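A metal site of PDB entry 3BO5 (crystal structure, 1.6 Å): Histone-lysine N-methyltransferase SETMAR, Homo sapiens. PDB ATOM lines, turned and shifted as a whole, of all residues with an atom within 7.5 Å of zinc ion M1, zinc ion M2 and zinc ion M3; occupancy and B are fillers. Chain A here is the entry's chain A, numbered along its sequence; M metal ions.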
ATOM      1  N   PRO A  60     -31.185 -10.896 -15.658  1.00  0.00           N
ATOM      2  CA  PRO A  60     -31.630  -9.494 -15.726  1.00  0.00           C
ATOM      3  C   PRO A  60     -31.298  -8.746 -17.014  1.00  0.00           C
ATOM      4  O   PRO A  60     -31.849  -7.657 -17.238  1.00  0.00           O
ATOM      5  CB  PRO A  60     -30.896  -8.815 -14.600  1.00  0.00           C
ATOM      6  CG  PRO A  60     -29.759  -9.655 -14.246  1.00  0.00           C
ATOM      7  CD  PRO A  60     -30.121 -11.110 -14.654  1.00  0.00           C
ATOM      8  N   GLY A  61     -30.465  -9.383 -17.798  1.00  0.00           N
ATOM      9  CA  GLY A  61     -30.128  -8.817 -19.136  1.00  0.00           C
ATOM     10  C   GLY A  61     -28.920  -7.894 -19.126  1.00  0.00           C
ATOM     11  O   GLY A  61     -28.240  -7.677 -18.092  1.00  0.00           O
ATOM     12  N   CYS A  62     -28.652  -7.314 -20.311  1.00  0.00           N
ATOM     13  CA  CYS A  62     -27.519  -6.399 -20.419  1.00  0.00           C
ATOM     14  C   CYS A  62     -28.002  -4.980 -20.262  1.00  0.00           C
ATOM     15  O   CYS A  62     -29.205  -4.666 -20.255  1.00  0.00           O
ATOM     16  CB  CYS A  62     -26.881  -6.582 -21.781  1.00  0.00           C
ATOM     17  SG  CYS A  62     -27.982  -6.197 -23.175  1.00  0.00           S
ATOM     18  N   ILE A  63     -26.975  -4.089 -20.166  1.00  0.00           N
ATOM     19  CA  ILE A  63     -27.327  -2.697 -19.925  1.00  0.00           C
ATOM     20  C   ILE A  63     -27.269  -1.825 -21.163  1.00  0.00           C
ATOM     21  O   ILE A  63     -27.446  -0.620 -21.060  1.00  0.00           O
ATOM     22  CB  ILE A  63     -26.417  -2.044 -18.853  1.00  0.00           C
ATOM     23  CG1 ILE A  63     -24.971  -1.956 -19.320  1.00  0.00           C
ATOM     24  CG2 ILE A  63     -26.555  -2.819 -17.511  1.00  0.00           C
ATOM     25  CD1 ILE A  63     -24.023  -1.184 -18.331  1.00  0.00           C
ATOM     26  N   CYS A  64     -27.131  -2.439 -22.319  1.00  0.00           N
ATOM     27  CA  CYS A  64     -26.917  -1.672 -23.539  1.00  0.00           C
ATOM     28  C   CYS A  64     -28.215  -1.030 -23.901  1.00  0.00           C
ATOM     29  O   CYS A  64     -29.279  -1.686 -23.855  1.00  0.00           O
ATOM     30  CB  CYS A  64     -26.567  -2.645 -24.650  1.00  0.00           C
ATOM     31  SG  CYS A  64     -25.266  -3.773 -24.158  1.00  0.00           S
ATOM     32  N   VAL A  65     -28.174   0.274 -24.127  1.00  0.00           N
ATOM     33  CA  VAL A  65     -29.380   0.906 -24.680  1.00  0.00           C
ATOM     34  C   VAL A  65     -28.996   1.963 -25.682  1.00  0.00           C
ATOM     35  O   VAL A  65     -29.649   2.074 -26.734  1.00  0.00           O
ATOM     36  CB  VAL A  65     -30.284   1.503 -23.608  1.00  0.00           C
ATOM     37  CG1 VAL A  65     -29.532   2.571 -22.765  1.00  0.00           C
ATOM     38  CG2 VAL A  65     -31.645   2.000 -24.313  1.00  0.00           C
ATOM     39  N   THR A  67     -26.204   2.103 -27.596  1.00  0.00           N
ATOM     40  CA  THR A  67     -25.503   1.615 -28.808  1.00  0.00           C
ATOM     41  C   THR A  67     -25.742   0.127 -28.880  1.00  0.00           C
ATOM     42  O   THR A  67     -26.150  -0.457 -27.871  1.00  0.00           O
ATOM     43  CB  THR A  67     -23.942   1.864 -28.746  1.00  0.00           C
ATOM     44  OG1 THR A  67     -23.415   1.221 -27.581  1.00  0.00           O
ATOM     45  CG2 THR A  67     -23.650   3.364 -28.651  1.00  0.00           C
ATOM     46  N   PRO A  68     -25.494  -0.481 -30.044  1.00  0.00           N
ATOM     47  CA  PRO A  68     -25.774  -1.914 -30.158  1.00  0.00           C
ATOM     48  C   PRO A  68     -24.958  -2.771 -29.190  1.00  0.00           C
ATOM     49  O   PRO A  68     -23.875  -2.420 -28.696  1.00  0.00           O
ATOM     50  CB  PRO A  68     -25.357  -2.248 -31.601  1.00  0.00           C
ATOM     51  CG  PRO A  68     -25.633  -0.892 -32.346  1.00  0.00           C
ATOM     52  CD  PRO A  68     -25.146   0.134 -31.352  1.00  0.00           C
ATOM     53  N   CYS A  69     -25.512  -3.967 -28.976  1.00  0.00           N
ATOM     54  CA  CYS A  69     -24.864  -4.908 -28.165  1.00  0.00           C
ATOM     55  C   CYS A  69     -23.637  -5.434 -28.927  1.00  0.00           C
ATOM     56  O   CYS A  69     -23.751  -6.037 -30.012  1.00  0.00           O
ATOM     57  CB  CYS A  69     -25.844  -6.065 -27.872  1.00  0.00           C
ATOM     58  SG  CYS A  69     -27.199  -5.485 -26.875  1.00  0.00           S
ATOM     59  N   LEU A  70     -22.518  -5.237 -28.298  1.00  0.00           N
ATOM     60  CA  LEU A  70     -21.251  -5.746 -28.871  1.00  0.00           C
ATOM     61  C   LEU A  70     -20.379  -6.355 -27.794  1.00  0.00           C
ATOM     62  O   LEU A  70     -20.441  -5.991 -26.593  1.00  0.00           O
ATOM     63  CB  LEU A  70     -20.531  -4.632 -29.630  1.00  0.00           C
ATOM     64  CG  LEU A  70     -21.192  -4.183 -30.945  1.00  0.00           C
ATOM     65  CD1 LEU A  70     -20.649  -2.785 -31.270  1.00  0.00           C
ATOM     66  CD2 LEU A  70     -20.941  -5.141 -32.065  1.00  0.00           C
ATOM     67  N   THR A  73     -18.817  -4.824 -24.202  1.00  0.00           N
ATOM     68  CA  THR A  73     -19.684  -3.858 -23.509  1.00  0.00           C
ATOM     69  C   THR A  73     -21.066  -4.479 -23.190  1.00  0.00           C
ATOM     70  O   THR A  73     -21.839  -3.953 -22.407  1.00  0.00           O
ATOM     71  CB  THR A  73     -19.830  -2.554 -24.282  1.00  0.00           C
ATOM     72  OG1 THR A  73     -20.273  -2.829 -25.608  1.00  0.00           O
ATOM     73  CG2 THR A  73     -18.455  -1.885 -24.451  1.00  0.00           C
ATOM     74  N   CYS A  74     -21.338  -5.629 -23.782  1.00  0.00           N
ATOM     75  CA  CYS A  74     -22.636  -6.284 -23.608  1.00  0.00           C
ATOM     76  C   CYS A  74     -22.460  -7.501 -22.757  1.00  0.00           C
ATOM     77  O   CYS A  74     -21.698  -8.416 -23.122  1.00  0.00           O
ATOM     78  CB  CYS A  74     -23.186  -6.697 -24.964  1.00  0.00           C
ATOM     79  SG  CYS A  74     -24.753  -7.581 -24.733  1.00  0.00           S
ATOM     80  N   SER A  75     -23.085  -7.486 -21.579  1.00  0.00           N
ATOM     81  CA  SER A  75     -22.919  -8.645 -20.654  1.00  0.00           C
ATOM     82  C   SER A  75     -23.572  -9.913 -21.161  1.00  0.00           C
ATOM     83  O   SER A  75     -23.341 -11.014 -20.663  1.00  0.00           O
ATOM     84  CB  SER A  75     -23.394  -8.333 -19.226  1.00  0.00           C
ATOM     85  OG  SER A  75     -24.723  -7.840 -19.202  1.00  0.00           O
ATOM     86  N   CYS A  76     -24.413  -9.774 -22.177  1.00  0.00           N
ATOM     87  CA  CYS A  76     -24.932 -10.957 -22.881  1.00  0.00           C
ATOM     88  C   CYS A  76     -23.952 -11.590 -23.878  1.00  0.00           C
ATOM     89  O   CYS A  76     -24.253 -12.693 -24.383  1.00  0.00           O
ATOM     90  CB  CYS A  76     -26.254 -10.638 -23.622  1.00  0.00           C
ATOM     91  SG  CYS A  76     -27.524 -10.076 -22.545  1.00  0.00           S
ATOM     92  N   LEU A  77     -22.857 -10.909 -24.196  1.00  0.00           N
ATOM     93  CA  LEU A  77     -21.916 -11.327 -25.210  1.00  0.00           C
ATOM     94  C   LEU A  77     -20.541 -11.525 -24.622  1.00  0.00           C
ATOM     95  O   LEU A  77     -19.549 -11.101 -25.232  1.00  0.00           O
ATOM     96  CB  LEU A  77     -21.806 -10.285 -26.318  1.00  0.00           C
ATOM     97  CG  LEU A  77     -23.082 -10.152 -27.136  1.00  0.00           C
ATOM     98  CD1 LEU A  77     -22.936  -9.136 -28.290  1.00  0.00           C
ATOM     99  CD2 LEU A  77     -23.517 -11.469 -27.698  1.00  0.00           C
ATOM    100  N   PHE A 103     -25.850 -16.971 -24.520  1.00  0.00           N
ATOM    101  CA  PHE A 103     -26.974 -16.203 -23.987  1.00  0.00           C
ATOM    102  C   PHE A 103     -27.451 -15.254 -25.051  1.00  0.00           C
ATOM    103  O   PHE A 103     -26.659 -14.542 -25.593  1.00  0.00           O
ATOM    104  CB  PHE A 103     -26.507 -15.395 -22.767  1.00  0.00           C
ATOM    105  CG  PHE A 103     -26.243 -16.253 -21.597  1.00  0.00           C
ATOM    106  CD1 PHE A 103     -27.240 -16.448 -20.630  1.00  0.00           C
ATOM    107  CD2 PHE A 103     -24.983 -16.864 -21.449  1.00  0.00           C
ATOM    108  CE1 PHE A 103     -27.009 -17.277 -19.517  1.00  0.00           C
ATOM    109  CE2 PHE A 103     -24.739 -17.696 -20.318  1.00  0.00           C
ATOM    110  CZ  PHE A 103     -25.733 -17.875 -19.390  1.00  0.00           C
ATOM    111  N   GLU A 104     -28.733 -15.292 -25.363  1.00  0.00           N
ATOM    112  CA  GLU A 104     -29.356 -14.219 -26.189  1.00  0.00           C
ATOM    113  C   GLU A 104     -29.780 -13.037 -25.314  1.00  0.00           C
ATOM    114  O   GLU A 104     -30.071 -13.195 -24.111  1.00  0.00           O
ATOM    115  CB  GLU A 104     -30.592 -14.748 -26.957  1.00  0.00           C
ATOM    116  CG  GLU A 104     -30.146 -15.735 -28.000  1.00  0.00           C
ATOM    117  CD  GLU A 104     -31.193 -15.978 -29.105  1.00  0.00           C
ATOM    118  OE1 GLU A 104     -32.342 -15.425 -29.063  1.00  0.00           O
ATOM    119  OE2 GLU A 104     -30.811 -16.813 -29.957  1.00  0.00           O
ATOM    120  N   CYS A 105     -29.904 -11.853 -25.955  1.00  0.00           N
ATOM    121  CA  CYS A 105     -30.570 -10.754 -25.262  1.00  0.00           C
ATOM    122  C   CYS A 105     -32.035 -11.179 -25.045  1.00  0.00           C
ATOM    123  O   CYS A 105     -32.571 -11.995 -25.769  1.00  0.00           O
ATOM    124  CB  CYS A 105     -30.411  -9.485 -26.053  1.00  0.00           C
ATOM    125  SG  CYS A 105     -28.766  -8.918 -25.973  1.00  0.00           S
ATOM    126  N   ASN A 106     -32.598 -10.718 -23.910  1.00  0.00           N
ATOM    127  CA  ASN A 106     -33.863 -11.220 -23.459  1.00  0.00           C
ATOM    128  C   ASN A 106     -34.894 -10.127 -23.238  1.00  0.00           C
ATOM    129  O   ASN A 106     -34.725  -9.023 -23.698  1.00  0.00           O
ATOM    130  CB  ASN A 106     -33.696 -12.137 -22.252  1.00  0.00           C
ATOM    131  CG  ASN A 106     -33.268 -11.395 -21.004  1.00  0.00           C
ATOM    132  OD1 ASN A 106     -33.473 -10.202 -20.875  1.00  0.00           O
ATOM    133  ND2 ASN A 106     -32.729 -12.140 -20.014  1.00  0.00           N
ATOM    134  N   LEU A 108     -35.639  -8.446 -20.817  1.00  0.00           N
ATOM    135  CA  LEU A 108     -35.206  -7.358 -19.972  1.00  0.00           C
ATOM    136  C   LEU A 108     -34.095  -6.501 -20.544  1.00  0.00           C
ATOM    137  O   LEU A 108     -33.763  -5.394 -19.968  1.00  0.00           O
ATOM    138  CB  LEU A 108     -34.800  -7.888 -18.626  1.00  0.00           C
ATOM    139  CG  LEU A 108     -35.975  -8.587 -17.938  1.00  0.00           C
ATOM    140  CD1 LEU A 108     -35.372  -8.948 -16.587  1.00  0.00           C
ATOM    141  CD2 LEU A 108     -37.242  -7.723 -17.808  1.00  0.00           C
ATOM    142  N   CYS A 109     -33.423  -6.978 -21.594  1.00  0.00           N
ATOM    143  CA  CYS A 109     -32.382  -6.204 -22.252  1.00  0.00           C
ATOM    144  C   CYS A 109     -33.078  -4.997 -22.915  1.00  0.00           C
ATOM    145  O   CYS A 109     -34.077  -5.185 -23.564  1.00  0.00           O
ATOM    146  CB  CYS A 109     -31.665  -7.099 -23.302  1.00  0.00           C
ATOM    147  SG  CYS A 109     -30.754  -8.445 -22.529  1.00  0.00           S
ATOM    148  N   ARG A 110     -32.438  -3.831 -22.861  1.00  0.00           N
ATOM    149  CA  ARG A 110     -33.102  -2.687 -23.459  1.00  0.00           C
ATOM    150  C   ARG A 110     -32.663  -2.445 -24.863  1.00  0.00           C
ATOM    151  O   ARG A 110     -33.231  -1.553 -25.514  1.00  0.00           O
ATOM    152  CB  ARG A 110     -32.879  -1.456 -22.622  1.00  0.00           C
ATOM    153  CG  ARG A 110     -33.717  -1.547 -21.370  1.00  0.00           C
ATOM    154  CD  ARG A 110     -33.005  -0.956 -20.186  1.00  0.00           C
ATOM    155  NE  ARG A 110     -32.929   0.464 -20.370  1.00  0.00           N
ATOM    156  CZ  ARG A 110     -32.352   1.301 -19.524  1.00  0.00           C
ATOM    157  NH1 ARG A 110     -32.337   2.610 -19.808  1.00  0.00           N
ATOM    158  NH2 ARG A 110     -31.795   0.836 -18.411  1.00  0.00           N
ATOM    159  N   CYS A 111     -31.736  -3.271 -25.374  1.00  0.00           N
ATOM    160  CA  CYS A 111     -31.491  -3.235 -26.812  1.00  0.00           C
ATOM    161  C   CYS A 111     -32.768  -3.494 -27.615  1.00  0.00           C
ATOM    162  O   CYS A 111     -33.724  -4.122 -27.110  1.00  0.00           O
ATOM    163  CB  CYS A 111     -30.398  -4.232 -27.224  1.00  0.00           C
ATOM    164  SG  CYS A 111     -30.912  -5.927 -26.691  1.00  0.00           S
ATOM    165  N   SER A 112     -32.812  -3.063 -28.865  1.00  0.00           N
ATOM    166  CA  SER A 112     -34.035  -3.214 -29.635  1.00  0.00           C
ATOM    167  C   SER A 112     -34.275  -4.631 -30.039  1.00  0.00           C
ATOM    168  O   SER A 112     -33.365  -5.505 -29.940  1.00  0.00           O
ATOM    169  CB  SER A 112     -34.046  -2.366 -30.898  1.00  0.00           C
ATOM    170  OG  SER A 112     -33.284  -2.996 -31.897  1.00  0.00           O
ATOM    171  N   HIS A 114     -34.244  -5.626 -32.797  1.00  0.00           N
ATOM    172  CA  HIS A 114     -33.324  -5.828 -33.934  1.00  0.00           C
ATOM    173  C   HIS A 114     -31.918  -6.235 -33.554  1.00  0.00           C
ATOM    174  O   HIS A 114     -31.019  -6.428 -34.395  1.00  0.00           O
ATOM    175  CB  HIS A 114     -33.350  -4.623 -34.846  1.00  0.00           C
ATOM    176  CG  HIS A 114     -34.736  -4.288 -35.287  1.00  0.00           C
ATOM    177  ND1 HIS A 114     -35.425  -3.178 -34.844  1.00  0.00           N
ATOM    178  CD2 HIS A 114     -35.619  -4.998 -36.040  1.00  0.00           C
ATOM    179  CE1 HIS A 114     -36.642  -3.174 -35.350  1.00  0.00           C
ATOM    180  NE2 HIS A 114     -36.793  -4.275 -36.082  1.00  0.00           N
ATOM    181  N   CYS A 115     -31.697  -6.358 -32.251  1.00  0.00           N
ATOM    182  CA  CYS A 115     -30.386  -6.678 -31.792  1.00  0.00           C
ATOM    183  C   CYS A 115     -29.957  -7.994 -32.468  1.00  0.00           C
ATOM    184  O   CYS A 115     -30.737  -8.945 -32.529  1.00  0.00           O
ATOM    185  CB  CYS A 115     -30.433  -6.910 -30.264  1.00  0.00           C
ATOM    186  SG  CYS A 115     -28.866  -7.480 -29.552  1.00  0.00           S
ATOM    187  N   ARG A 116     -28.701  -8.036 -32.926  1.00  0.00           N
ATOM    188  CA  ARG A 116     -28.153  -9.246 -33.577  1.00  0.00           C
ATOM    189  C   ARG A 116     -28.040 -10.435 -32.650  1.00  0.00           C
ATOM    190  O   ARG A 116     -27.869 -11.557 -33.170  1.00  0.00           O
ATOM    191  CB  ARG A 116     -26.788  -9.008 -34.225  1.00  0.00           C
ATOM    192  CG  ARG A 116     -27.020  -8.199 -35.519  1.00  0.00           C
ATOM    193  CD  ARG A 116     -25.796  -7.371 -35.877  1.00  0.00           C
ATOM    194  NE  ARG A 116     -24.627  -8.138 -36.298  1.00  0.00           N
ATOM    195  CZ  ARG A 116     -23.518  -7.564 -36.760  1.00  0.00           C
ATOM    196  NH1 ARG A 116     -22.489  -8.301 -37.136  1.00  0.00           N
ATOM    197  NH2 ARG A 116     -23.452  -6.236 -36.846  1.00  0.00           N
ATOM    198  N   ASN A 117     -28.149 -10.196 -31.344  1.00  0.00           N
ATOM    199  CA  ASN A 117     -28.093 -11.312 -30.400  1.00  0.00           C
ATOM    200  C   ASN A 117     -29.487 -11.776 -29.983  1.00  0.00           C
ATOM    201  O   ASN A 117     -29.626 -12.337 -28.885  1.00  0.00           O
ATOM    202  CB  ASN A 117     -27.234 -10.949 -29.160  1.00  0.00           C
ATOM    203  CG  ASN A 117     -26.825 -12.135 -28.378  1.00  0.00           C
ATOM    204  OD1 ASN A 117     -26.367 -13.117 -28.955  1.00  0.00           O
ATOM    205  ND2 ASN A 117     -26.889 -12.021 -27.051  1.00  0.00           N
ATOM    206  N   ARG A 118     -30.480 -11.564 -30.862  1.00  0.00           N
ATOM    207  CA  ARG A 118     -31.848 -12.144 -30.689  1.00  0.00           C
ATOM    208  C   ARG A 118     -32.096 -12.938 -31.947  1.00  0.00           C
ATOM    209  O   ARG A 118     -32.249 -12.344 -33.032  1.00  0.00           O
ATOM    210  CB  ARG A 118     -32.903 -11.031 -30.544  1.00  0.00           C
ATOM    211  CG  ARG A 118     -32.619 -10.097 -29.381  1.00  0.00           C
ATOM    212  CD  ARG A 118     -33.594  -8.977 -29.428  1.00  0.00           C
ATOM    213  NE  ARG A 118     -33.474  -8.008 -28.314  1.00  0.00           N
ATOM    214  CZ  ARG A 118     -33.990  -8.152 -27.116  1.00  0.00           C
ATOM    215  NH1 ARG A 118     -34.557  -9.293 -26.747  1.00  0.00           N
ATOM    216  NH2 ARG A 118     -33.865  -7.125 -26.228  1.00  0.00           N
HETATM  217 ZN    ZN M   1     -28.675  -8.430 -23.667  1.00  0.00          ZN
HETATM  218 ZN    ZN M   2     -28.969  -6.980 -27.318  1.00  0.00          ZN
HETATM  219 ZN    ZN M   3     -26.213  -5.837 -24.701  1.00  0.00          ZN
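The side-chain sulfur (SG) of Cys 115 binds zinc ion M2 (2.3 Å).
Zinc ion M2 is bound by the side-chain sulfur (SG) of Cys 111 (2.3 Å).
SG of Cys 69 binds zinc ion M2, at 2.4 Å.
Zinc ion M2 is bound by the side-chain sulfur (SG) of Cys 105 (2.4 Å).
Within 4 Å of zinc ion M1: Cys 62, Cys 76, Cys 105 and Cys 109.
The nearest printed residue that does not touch zinc ion M1 is Cys 74 (4.2 Å).
Zinc ion M3 is bound by the side-chain sulfur of Cys 74 (2.3 Å), the side-chain sulfur of Cys 64 (2.3 Å), the side-chain sulfur of Cys 62 (2.4 Å) and the side-chain sulfur of Cys 69 (2.4 Å).
Zinc ion M3 has four donor atoms within binding distance.
The side-chain sulfur (SG) of Cys 74 sits close to the backbone NH (N) of Cys 76, at 3.4 Å.
The side-chain sulfur of Cys 115 lies close to the backbone NH of Asn 117 (3.3 Å).
The backbone NH of Cys 111 is in hydrogen-bond range of the backbone carbonyl oxygen of Cys 64, at 3.3 Å.
O of Cys 111 sits at hydrogen-bond distance from NH2 of Arg 118 (3.1 Å).
The backbone carbonyl oxygen (O) of Asn 117 sits at hydrogen-bond distance from the backbone NH (N) of Cys 105, at 3.0 Å.
O of Cys 105 sits at hydrogen-bond distance from NH1 of Arg 118 (3.5 Å).
The backbone NH (N) of Cys 109 lies within hydrogen-bond range of the side-chain amide oxygen (OD1) of Asn 106, at 3.3 Å.
The backbone carbonyl oxygen (O) of Cys 109 is in hydrogen-bond range of the guanidinium group (NH2) of Arg 118, at 3.3 Å.
Four residues have an atom within 4 Å of zinc ion M3: Cys 62, Cys 64, Cys 69 and Cys 74.
The nearest printed residue that does not touch zinc ion M3 is Cys 105 (4.2 Å).
Zinc ion M1 is bound by SG of Cys 76 (2.3 Å), SG of Cys 105 (2.4 Å), SG of Cys 109 (2.4 Å) and SG of Cys 62 (2.4 Å).
Four residues have an atom within 4 Å of zinc ion M2: Cys 69, Cys 105, Cys 111 and Cys 115.
The nearest printed residue that does not touch zinc ion M2 is Cys 62 (4.3 Å).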
